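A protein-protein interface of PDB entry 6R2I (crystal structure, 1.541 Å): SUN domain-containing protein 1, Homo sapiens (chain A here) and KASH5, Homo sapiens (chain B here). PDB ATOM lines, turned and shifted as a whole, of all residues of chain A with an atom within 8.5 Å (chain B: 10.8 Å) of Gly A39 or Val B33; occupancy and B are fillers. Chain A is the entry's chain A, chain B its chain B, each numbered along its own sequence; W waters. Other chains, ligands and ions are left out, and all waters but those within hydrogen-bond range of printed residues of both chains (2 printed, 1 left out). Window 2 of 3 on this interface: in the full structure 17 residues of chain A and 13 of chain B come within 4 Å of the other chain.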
ATOM      1  N   VAL A  32       4.421 -34.750 -21.289  1.00  0.00           N
ATOM      2  CA  VAL A  32       5.779 -34.220 -21.465  1.00  0.00           C
ATOM      3  C   VAL A  32       5.985 -33.008 -20.550  1.00  0.00           C
ATOM      4  O   VAL A  32       5.142 -32.095 -20.510  1.00  0.00           O
ATOM      5  CB  VAL A  32       6.068 -33.810 -22.925  1.00  0.00           C
ATOM      6  CG1 VAL A  32       7.502 -33.238 -23.059  1.00  0.00           C
ATOM      7  CG2 VAL A  32       5.874 -34.980 -23.880  1.00  0.00           C
ATOM      8  N   ASP A  33       7.170 -32.941 -19.896  1.00  0.00           N
ATOM      9  CA  ASP A  33       7.637 -31.762 -19.147  1.00  0.00           C
ATOM     10  C   ASP A  33       8.778 -31.106 -19.942  1.00  0.00           C
ATOM     11  O   ASP A  33       9.914 -31.616 -19.949  1.00  0.00           O
ATOM     12  CB  ASP A  33       8.121 -32.134 -17.755  1.00  0.00           C
ATOM     13  CG  ASP A  33       8.686 -30.937 -16.985  1.00  0.00           C
ATOM     14  OD1 ASP A  33       8.557 -29.787 -17.464  1.00  0.00           O
ATOM     15  OD2 ASP A  33       9.286 -31.190 -15.910  1.00  0.00           O
ATOM     16  N   PHE A  34       8.474 -29.986 -20.624  1.00  0.00           N
ATOM     17  CA  PHE A  34       9.466 -29.286 -21.444  1.00  0.00           C
ATOM     18  C   PHE A  34      10.463 -28.471 -20.619  1.00  0.00           C
ATOM     19  O   PHE A  34      11.451 -27.953 -21.206  1.00  0.00           O
ATOM     20  CB  PHE A  34       8.755 -28.387 -22.472  1.00  0.00           C
ATOM     21  CG  PHE A  34       7.971 -29.169 -23.535  1.00  0.00           C
ATOM     22  CD1 PHE A  34       8.636 -29.730 -24.631  1.00  0.00           C
ATOM     23  CD2 PHE A  34       6.612 -29.352 -23.414  1.00  0.00           C
ATOM     24  CE1 PHE A  34       7.964 -30.465 -25.568  1.00  0.00           C
ATOM     25  CE2 PHE A  34       5.892 -30.096 -24.361  1.00  0.00           C
ATOM     26  CZ  PHE A  34       6.556 -30.643 -25.449  1.00  0.00           C
ATOM     27  N   ALA A  35      10.284 -28.390 -19.286  1.00  0.00           N
ATOM     28  CA  ALA A  35      11.286 -27.765 -18.408  1.00  0.00           C
ATOM     29  C   ALA A  35      12.322 -28.740 -17.849  1.00  0.00           C
ATOM     30  O   ALA A  35      13.382 -28.289 -17.395  1.00  0.00           O
ATOM     31  CB  ALA A  35      10.595 -27.046 -17.232  1.00  0.00           C
ATOM     32  N   LEU A  36      12.072 -30.044 -17.905  1.00  0.00           N
ATOM     33  CA  LEU A  36      12.923 -31.039 -17.242  1.00  0.00           C
ATOM     34  C   LEU A  36      14.359 -30.945 -17.754  1.00  0.00           C
ATOM     35  O   LEU A  36      14.607 -31.022 -18.952  1.00  0.00           O
ATOM     36  CB  LEU A  36      12.346 -32.438 -17.521  1.00  0.00           C
ATOM     37  CG  LEU A  36      13.052 -33.639 -16.883  1.00  0.00           C
ATOM     38  CD1 LEU A  36      12.772 -33.671 -15.389  1.00  0.00           C
ATOM     39  CD2 LEU A  36      12.649 -34.963 -17.563  1.00  0.00           C
ATOM     40  N   GLU A  37      15.322 -30.852 -16.824  1.00  0.00           N
ATOM     41  CA  GLU A  37      16.713 -30.610 -17.235  1.00  0.00           C
ATOM     42  C   GLU A  37      17.282 -31.763 -18.061  1.00  0.00           C
ATOM     43  O   GLU A  37      17.924 -31.534 -19.109  1.00  0.00           O
ATOM     44  CB  GLU A  37      17.591 -30.359 -16.005  1.00  0.00           C
ATOM     45  CG  GLU A  37      18.988 -29.824 -16.370  1.00  0.00           C
ATOM     46  CD  GLU A  37      19.857 -29.544 -15.154  1.00  0.00           C
ATOM     47  OE1 GLU A  37      20.183 -30.522 -14.425  1.00  0.00           O
ATOM     48  OE2 GLU A  37      20.213 -28.347 -14.919  1.00  0.00           O
ATOM     49  N   SER A  38      17.055 -33.019 -17.640  1.00  0.00           N
ATOM     50  CA  SER A  38      17.681 -34.128 -18.365  1.00  0.00           C
ATOM     51  C   SER A  38      17.183 -34.234 -19.814  1.00  0.00           C
ATOM     52  O   SER A  38      17.919 -34.728 -20.693  1.00  0.00           O
ATOM     53  CB  SER A  38      17.443 -35.439 -17.613  1.00  0.00           C
ATOM     54  OG  SER A  38      16.056 -35.765 -17.534  1.00  0.00           O
ATOM     55  N   GLY A  39      15.966 -33.769 -20.096  1.00  0.00           N
ATOM     56  CA  GLY A  39      15.431 -33.784 -21.440  1.00  0.00           C
ATOM     57  C   GLY A  39      15.734 -32.575 -22.298  1.00  0.00           C
ATOM     58  O   GLY A  39      15.310 -32.538 -23.472  1.00  0.00           O
ATOM     59  N   GLY A  40      16.430 -31.568 -21.749  1.00  0.00           N
ATOM     60  CA  GLY A  40      16.836 -30.398 -22.530  1.00  0.00           C
ATOM     61  C   GLY A  40      16.447 -29.025 -21.986  1.00  0.00           C
ATOM     62  O   GLY A  40      16.820 -27.992 -22.575  1.00  0.00           O
ATOM     63  N   GLY A  41      15.748 -28.992 -20.844  1.00  0.00           N
ATOM     64  CA  GLY A  41      15.495 -27.721 -20.153  1.00  0.00           C
ATOM     65  C   GLY A  41      16.738 -27.227 -19.403  1.00  0.00           C
ATOM     66  O   GLY A  41      17.623 -28.008 -19.067  1.00  0.00           O
ATOM     67  N   SER A  42      16.786 -25.923 -19.112  1.00  0.00           N
ATOM     68  CA  SER A  42      17.917 -25.381 -18.350  1.00  0.00           C
ATOM     69  C   SER A  42      17.530 -24.100 -17.632  1.00  0.00           C
ATOM     70  O   SER A  42      16.611 -23.384 -18.046  1.00  0.00           O
ATOM     71  CB  SER A  42      19.130 -25.129 -19.244  1.00  0.00           C
ATOM     72  OG  SER A  42      18.833 -24.212 -20.299  1.00  0.00           O
ATOM     73  N   ILE A  77      14.132 -28.266 -11.567  1.00  0.00           N
ATOM     74  CA  ILE A  77      13.831 -28.989 -12.804  1.00  0.00           C
ATOM     75  C   ILE A  77      14.473 -30.382 -12.793  1.00  0.00           C
ATOM     76  O   ILE A  77      14.803 -30.953 -13.853  1.00  0.00           O
ATOM     77  CB  ILE A  77      14.206 -28.141 -14.046  1.00  0.00           C
ATOM     78  CG1 ILE A  77      15.640 -27.637 -14.023  1.00  0.00           C
ATOM     79  CG2 ILE A  77      13.276 -26.892 -14.127  1.00  0.00           C
ATOM     80  CD1 ILE A  77      16.101 -27.067 -15.363  1.00  0.00           C
ATOM     81  N   ARG A  99      14.708 -22.025 -19.664  1.00  0.00           N
ATOM     82  CA  ARG A  99      14.678 -22.266 -21.109  1.00  0.00           C
ATOM     83  C   ARG A  99      14.153 -23.690 -21.359  1.00  0.00           C
ATOM     84  O   ARG A  99      14.655 -24.649 -20.776  1.00  0.00           O
ATOM     85  CB  ARG A  99      16.070 -22.089 -21.734  1.00  0.00           C
ATOM     86  CG  ARG A  99      16.061 -22.137 -23.246  1.00  0.00           C
ATOM     87  CD  ARG A  99      17.444 -21.992 -23.837  1.00  0.00           C
ATOM     88  NE  ARG A  99      17.498 -22.112 -25.297  1.00  0.00           N
ATOM     89  CZ  ARG A  99      17.470 -23.260 -25.977  1.00  0.00           C
ATOM     90  NH1 ARG A  99      17.330 -24.431 -25.351  1.00  0.00           N
ATOM     91  NH2 ARG A  99      17.573 -23.228 -27.312  1.00  0.00           N
ATOM     92  N   LEU A 100      13.161 -23.827 -22.227  1.00  0.00           N
ATOM     93  CA  LEU A 100      12.500 -25.106 -22.490  1.00  0.00           C
ATOM     94  C   LEU A 100      13.238 -25.911 -23.561  1.00  0.00           C
ATOM     95  O   LEU A 100      14.042 -25.378 -24.333  1.00  0.00           O
ATOM     96  CB  LEU A 100      11.054 -24.862 -22.939  1.00  0.00           C
ATOM     97  CG  LEU A 100      10.157 -23.959 -22.089  1.00  0.00           C
ATOM     98  CD1 LEU A 100       8.773 -23.824 -22.726  1.00  0.00           C
ATOM     99  CD2 LEU A 100      10.064 -24.510 -20.672  1.00  0.00           C
ATOM    100  N   SER A 101      12.983 -27.231 -23.566  1.00  0.00           N
ATOM    101  CA  SER A 101      13.625 -28.141 -24.519  1.00  0.00           C
ATOM    102  C   SER A 101      13.081 -28.019 -25.944  1.00  0.00           C
ATOM    103  O   SER A 101      13.728 -28.523 -26.881  1.00  0.00           O
ATOM    104  CB  SER A 101      13.502 -29.593 -24.032  1.00  0.00           C
ATOM    105  OG  SER A 101      12.142 -29.962 -23.905  1.00  0.00           O
ATOM    106  N   MET A 102      11.944 -27.359 -26.141  1.00  0.00           N
ATOM    107  CA  MET A 102      11.394 -27.117 -27.466  1.00  0.00           C
ATOM    108  C   MET A 102      10.608 -25.817 -27.411  1.00  0.00           C
ATOM    109  O   MET A 102      10.158 -25.402 -26.343  1.00  0.00           O
ATOM    110  CB  MET A 102      10.467 -28.251 -27.930  1.00  0.00           C
ATOM    111  CG  MET A 102      11.194 -29.517 -28.336  1.00  0.00           C
ATOM    112  SD  MET A 102      10.202 -30.526 -29.453  1.00  0.00           S
ATOM    113  CE  MET A 102      10.115 -29.424 -30.868  1.00  0.00           C
ATOM    114  N   LEU B  25      24.681 -25.596 -15.914  1.00  0.00           N
ATOM    115  CA  LEU B  25      24.495 -26.464 -17.068  1.00  0.00           C
ATOM    116  C   LEU B  25      23.678 -25.735 -18.121  1.00  0.00           C
ATOM    117  O   LEU B  25      22.568 -25.275 -17.836  1.00  0.00           O
ATOM    118  CB  LEU B  25      23.785 -27.768 -16.664  1.00  0.00           C
ATOM    119  CG  LEU B  25      23.575 -28.831 -17.747  1.00  0.00           C
ATOM    120  CD1 LEU B  25      23.291 -30.199 -17.131  1.00  0.00           C
ATOM    121  CD2 LEU B  25      22.435 -28.457 -18.685  1.00  0.00           C
ATOM    122  N   CYS B  26      24.199 -25.679 -19.349  1.00  0.00           N
ATOM    123  CA  CYS B  26      23.442 -25.138 -20.472  1.00  0.00           C
ATOM    124  C   CYS B  26      23.593 -26.028 -21.706  1.00  0.00           C
ATOM    125  O   CYS B  26      24.541 -26.805 -21.835  1.00  0.00           O
ATOM    126  CB  CYS B  26      23.880 -23.707 -20.774  1.00  0.00           C
ATOM    127  SG  CYS B  26      25.357 -23.574 -21.760  1.00  0.00           S
ATOM    128  N   TYR B  27      22.616 -25.919 -22.611  1.00  0.00           N
ATOM    129  CA  TYR B  27      22.542 -26.749 -23.809  1.00  0.00           C
ATOM    130  C   TYR B  27      22.720 -25.879 -25.050  1.00  0.00           C
ATOM    131  O   TYR B  27      21.907 -24.982 -25.305  1.00  0.00           O
ATOM    132  CB  TYR B  27      21.204 -27.494 -23.895  1.00  0.00           C
ATOM    133  CG  TYR B  27      21.027 -28.606 -22.888  1.00  0.00           C
ATOM    134  CD1 TYR B  27      21.773 -29.777 -22.975  1.00  0.00           C
ATOM    135  CD2 TYR B  27      20.099 -28.499 -21.863  1.00  0.00           C
ATOM    136  CE1 TYR B  27      21.612 -30.800 -22.056  1.00  0.00           C
ATOM    137  CE2 TYR B  27      19.933 -29.516 -20.942  1.00  0.00           C
ATOM    138  CZ  TYR B  27      20.685 -30.665 -21.044  1.00  0.00           C
ATOM    139  OH  TYR B  27      20.519 -31.683 -20.129  1.00  0.00           O
ATOM    140  N   GLN B  29      22.542 -27.326 -27.986  1.00  0.00           N
ATOM    141  CA  GLN B  29      21.465 -27.914 -28.767  1.00  0.00           C
ATOM    142  C   GLN B  29      20.858 -29.024 -27.931  1.00  0.00           C
ATOM    143  O   GLN B  29      21.440 -29.431 -26.921  1.00  0.00           O
ATOM    144  CB  GLN B  29      21.976 -28.468 -30.101  1.00  0.00           C
ATOM    145  CG  GLN B  29      22.942 -29.632 -29.946  1.00  0.00           C
ATOM    146  CD  GLN B  29      23.495 -30.096 -31.276  1.00  0.00           C
ATOM    147  OE1 GLN B  29      23.817 -29.279 -32.145  1.00  0.00           O
ATOM    148  NE2 GLN B  29      23.597 -31.413 -31.451  1.00  0.00           N
ATOM    149  N   PRO B  30      19.694 -29.534 -28.317  1.00  0.00           N
ATOM    150  CA  PRO B  30      19.005 -30.511 -27.476  1.00  0.00           C
ATOM    151  C   PRO B  30      19.819 -31.780 -27.282  1.00  0.00           C
ATOM    152  O   PRO B  30      20.440 -32.287 -28.225  1.00  0.00           O
ATOM    153  CB  PRO B  30      17.720 -30.806 -28.257  1.00  0.00           C
ATOM    154  CG  PRO B  30      17.500 -29.585 -29.106  1.00  0.00           C
ATOM    155  CD  PRO B  30      18.875 -29.137 -29.485  1.00  0.00           C
ATOM    156  N   PRO B  31      19.790 -32.360 -26.082  1.00  0.00           N
ATOM    157  CA  PRO B  31      20.470 -33.634 -25.852  1.00  0.00           C
ATOM    158  C   PRO B  31      19.701 -34.789 -26.461  1.00  0.00           C
ATOM    159  O   PRO B  31      18.474 -34.700 -26.637  1.00  0.00           O
ATOM    160  CB  PRO B  31      20.487 -33.744 -24.322  1.00  0.00           C
ATOM    161  CG  PRO B  31      19.244 -33.040 -23.906  1.00  0.00           C
ATOM    162  CD  PRO B  31      19.106 -31.882 -24.858  1.00  0.00           C
ATOM    163  N   PRO B  32      20.365 -35.914 -26.731  1.00  0.00           N
ATOM    164  CA  PRO B  32      19.630 -37.097 -27.194  1.00  0.00           C
ATOM    165  C   PRO B  32      18.603 -37.592 -26.180  1.00  0.00           C
ATOM    166  O   PRO B  32      18.868 -37.663 -24.971  1.00  0.00           O
ATOM    167  CB  PRO B  32      20.738 -38.139 -27.438  1.00  0.00           C
ATOM    168  CG  PRO B  32      22.019 -37.332 -27.637  1.00  0.00           C
ATOM    169  CD  PRO B  32      21.822 -36.142 -26.693  1.00  0.00           C
ATOM    170  N   VAL B  33      17.407 -37.931 -26.685  1.00  0.00           N
ATOM    171  CA  VAL B  33      16.351 -38.516 -25.837  1.00  0.00           C
ATOM    172  C   VAL B  33      15.717 -39.683 -26.575  1.00  0.00           C
ATOM    173  O   VAL B  33      15.911 -39.803 -27.809  1.00  0.00           O
ATOM    174  CB  VAL B  33      15.247 -37.495 -25.407  1.00  0.00           C
ATOM    175  CG1 VAL B  33      15.823 -36.320 -24.629  1.00  0.00           C
ATOM    176  CG2 VAL B  33      14.475 -36.979 -26.599  1.00  0.00           C
ATOM    177  OXT VAL B  33      14.956 -40.483 -25.989  1.00  0.00           O
HETATM  178  O   HOH W   1      20.682 -23.751 -22.245  1.00  0.00           O
HETATM  179  O   HOH W   2      20.391 -25.763 -15.984  1.00  0.00           O
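The backbone carbonyl oxygen of Glu A37 lies within hydrogen-bond range of the side-chain hydroxyl of Tyr B27, at 2.8 Å.
The backbone carbonyl oxygen (O) of Ser A42 lies within hydrogen-bond range of the backbone NH (N) of Arg A99, 2.8 Å away.
The backbone carbonyl oxygen (O) of Leu A36 lies within hydrogen-bond range of the backbone NH (N) of Gly A41, at 3.0 Å.
The backbone carbonyl oxygen (O) of Ile A77 lies within hydrogen-bond range of the backbone NH (N) of Glu A37, 3.0 Å away.
Among the printed residues, pairs that only touch across the chains: Ser A38 with Pro B31, Gly A39 with Pro B31, Gly A39 with Val B33, Gly A40 with Tyr B27, Gly A40 with Pro B31, Gly A41 with Tyr B27 and Ser A42 with Leu B25.
Printed residues of chain B within 4 Å of Gly A39: Pro B31 (3.9 Å) and Val B33 (3.99 Å).
Of the printed residues of chain A, Val B33 touches Gly A39 (3.99 Å).
No residue of chain B comes within 4 Å of Leu A36.
Printed residues of chain B within 4 Å of Ser A38: Pro B31.
Gly A40 touches just these residues of chain B: Tyr B27 (3.4 Å) and Pro B31 (3.6 Å).
Printed residues of chain A within 4 Å of Pro B31: Ser A38, Gly A39 and Gly A40.
Of the printed residues of chain A, Tyr B27 touches Glu A37 (2.8 Å), Gly A40 (3.4 Å) and Gly A41 (3.3 Å).
Of the printed residues of chain B, Ser A42 touches Leu B25 (3.7 Å).
Of the printed residues of chain A, Leu B25 touches Ser A42 (3.7 Å).
Arg A99 touches none of the printed residues of chain B.
Val A32 touches none of the printed residues of chain B.
The nearest printed residue of chain A that does not touch Leu B25 is Glu A37 (4.02 Å).
Of the 8 printed residues of chain B, 4 touch a printed residue of chain A.
Hydrophobic or aromatic side chains of chain B within 4 Å of the printed part of chain A: Tyr B27, Pro B31 and Val B33.
Along chain B the printed residues that touch a printed residue of chain A span positions 25 to 33.
Printed residues of chain A that touch a printed residue of chain B: Glu A37, Ser A38, Gly A39, Gly A40, Gly A41 and Ser A42.
Along chain A the printed residues that touch a printed residue of chain B span positions 37 to 42.
Among the printed residues, no Asp or Glu carboxylate lies within 4 Å of a Lys or Arg side-chain nitrogen of the other chain.
Water W1 bridges the side-chain hydroxyl of Ser A42 (2.7 Å) and the backbone NH of Tyr B27 (2.9 Å).
Water W2 lies within hydrogen-bond range of the side-chain carboxylate of Glu A37 (2.8 Å) and the backbone carbonyl oxygen of Leu B25 (2.9 Å).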
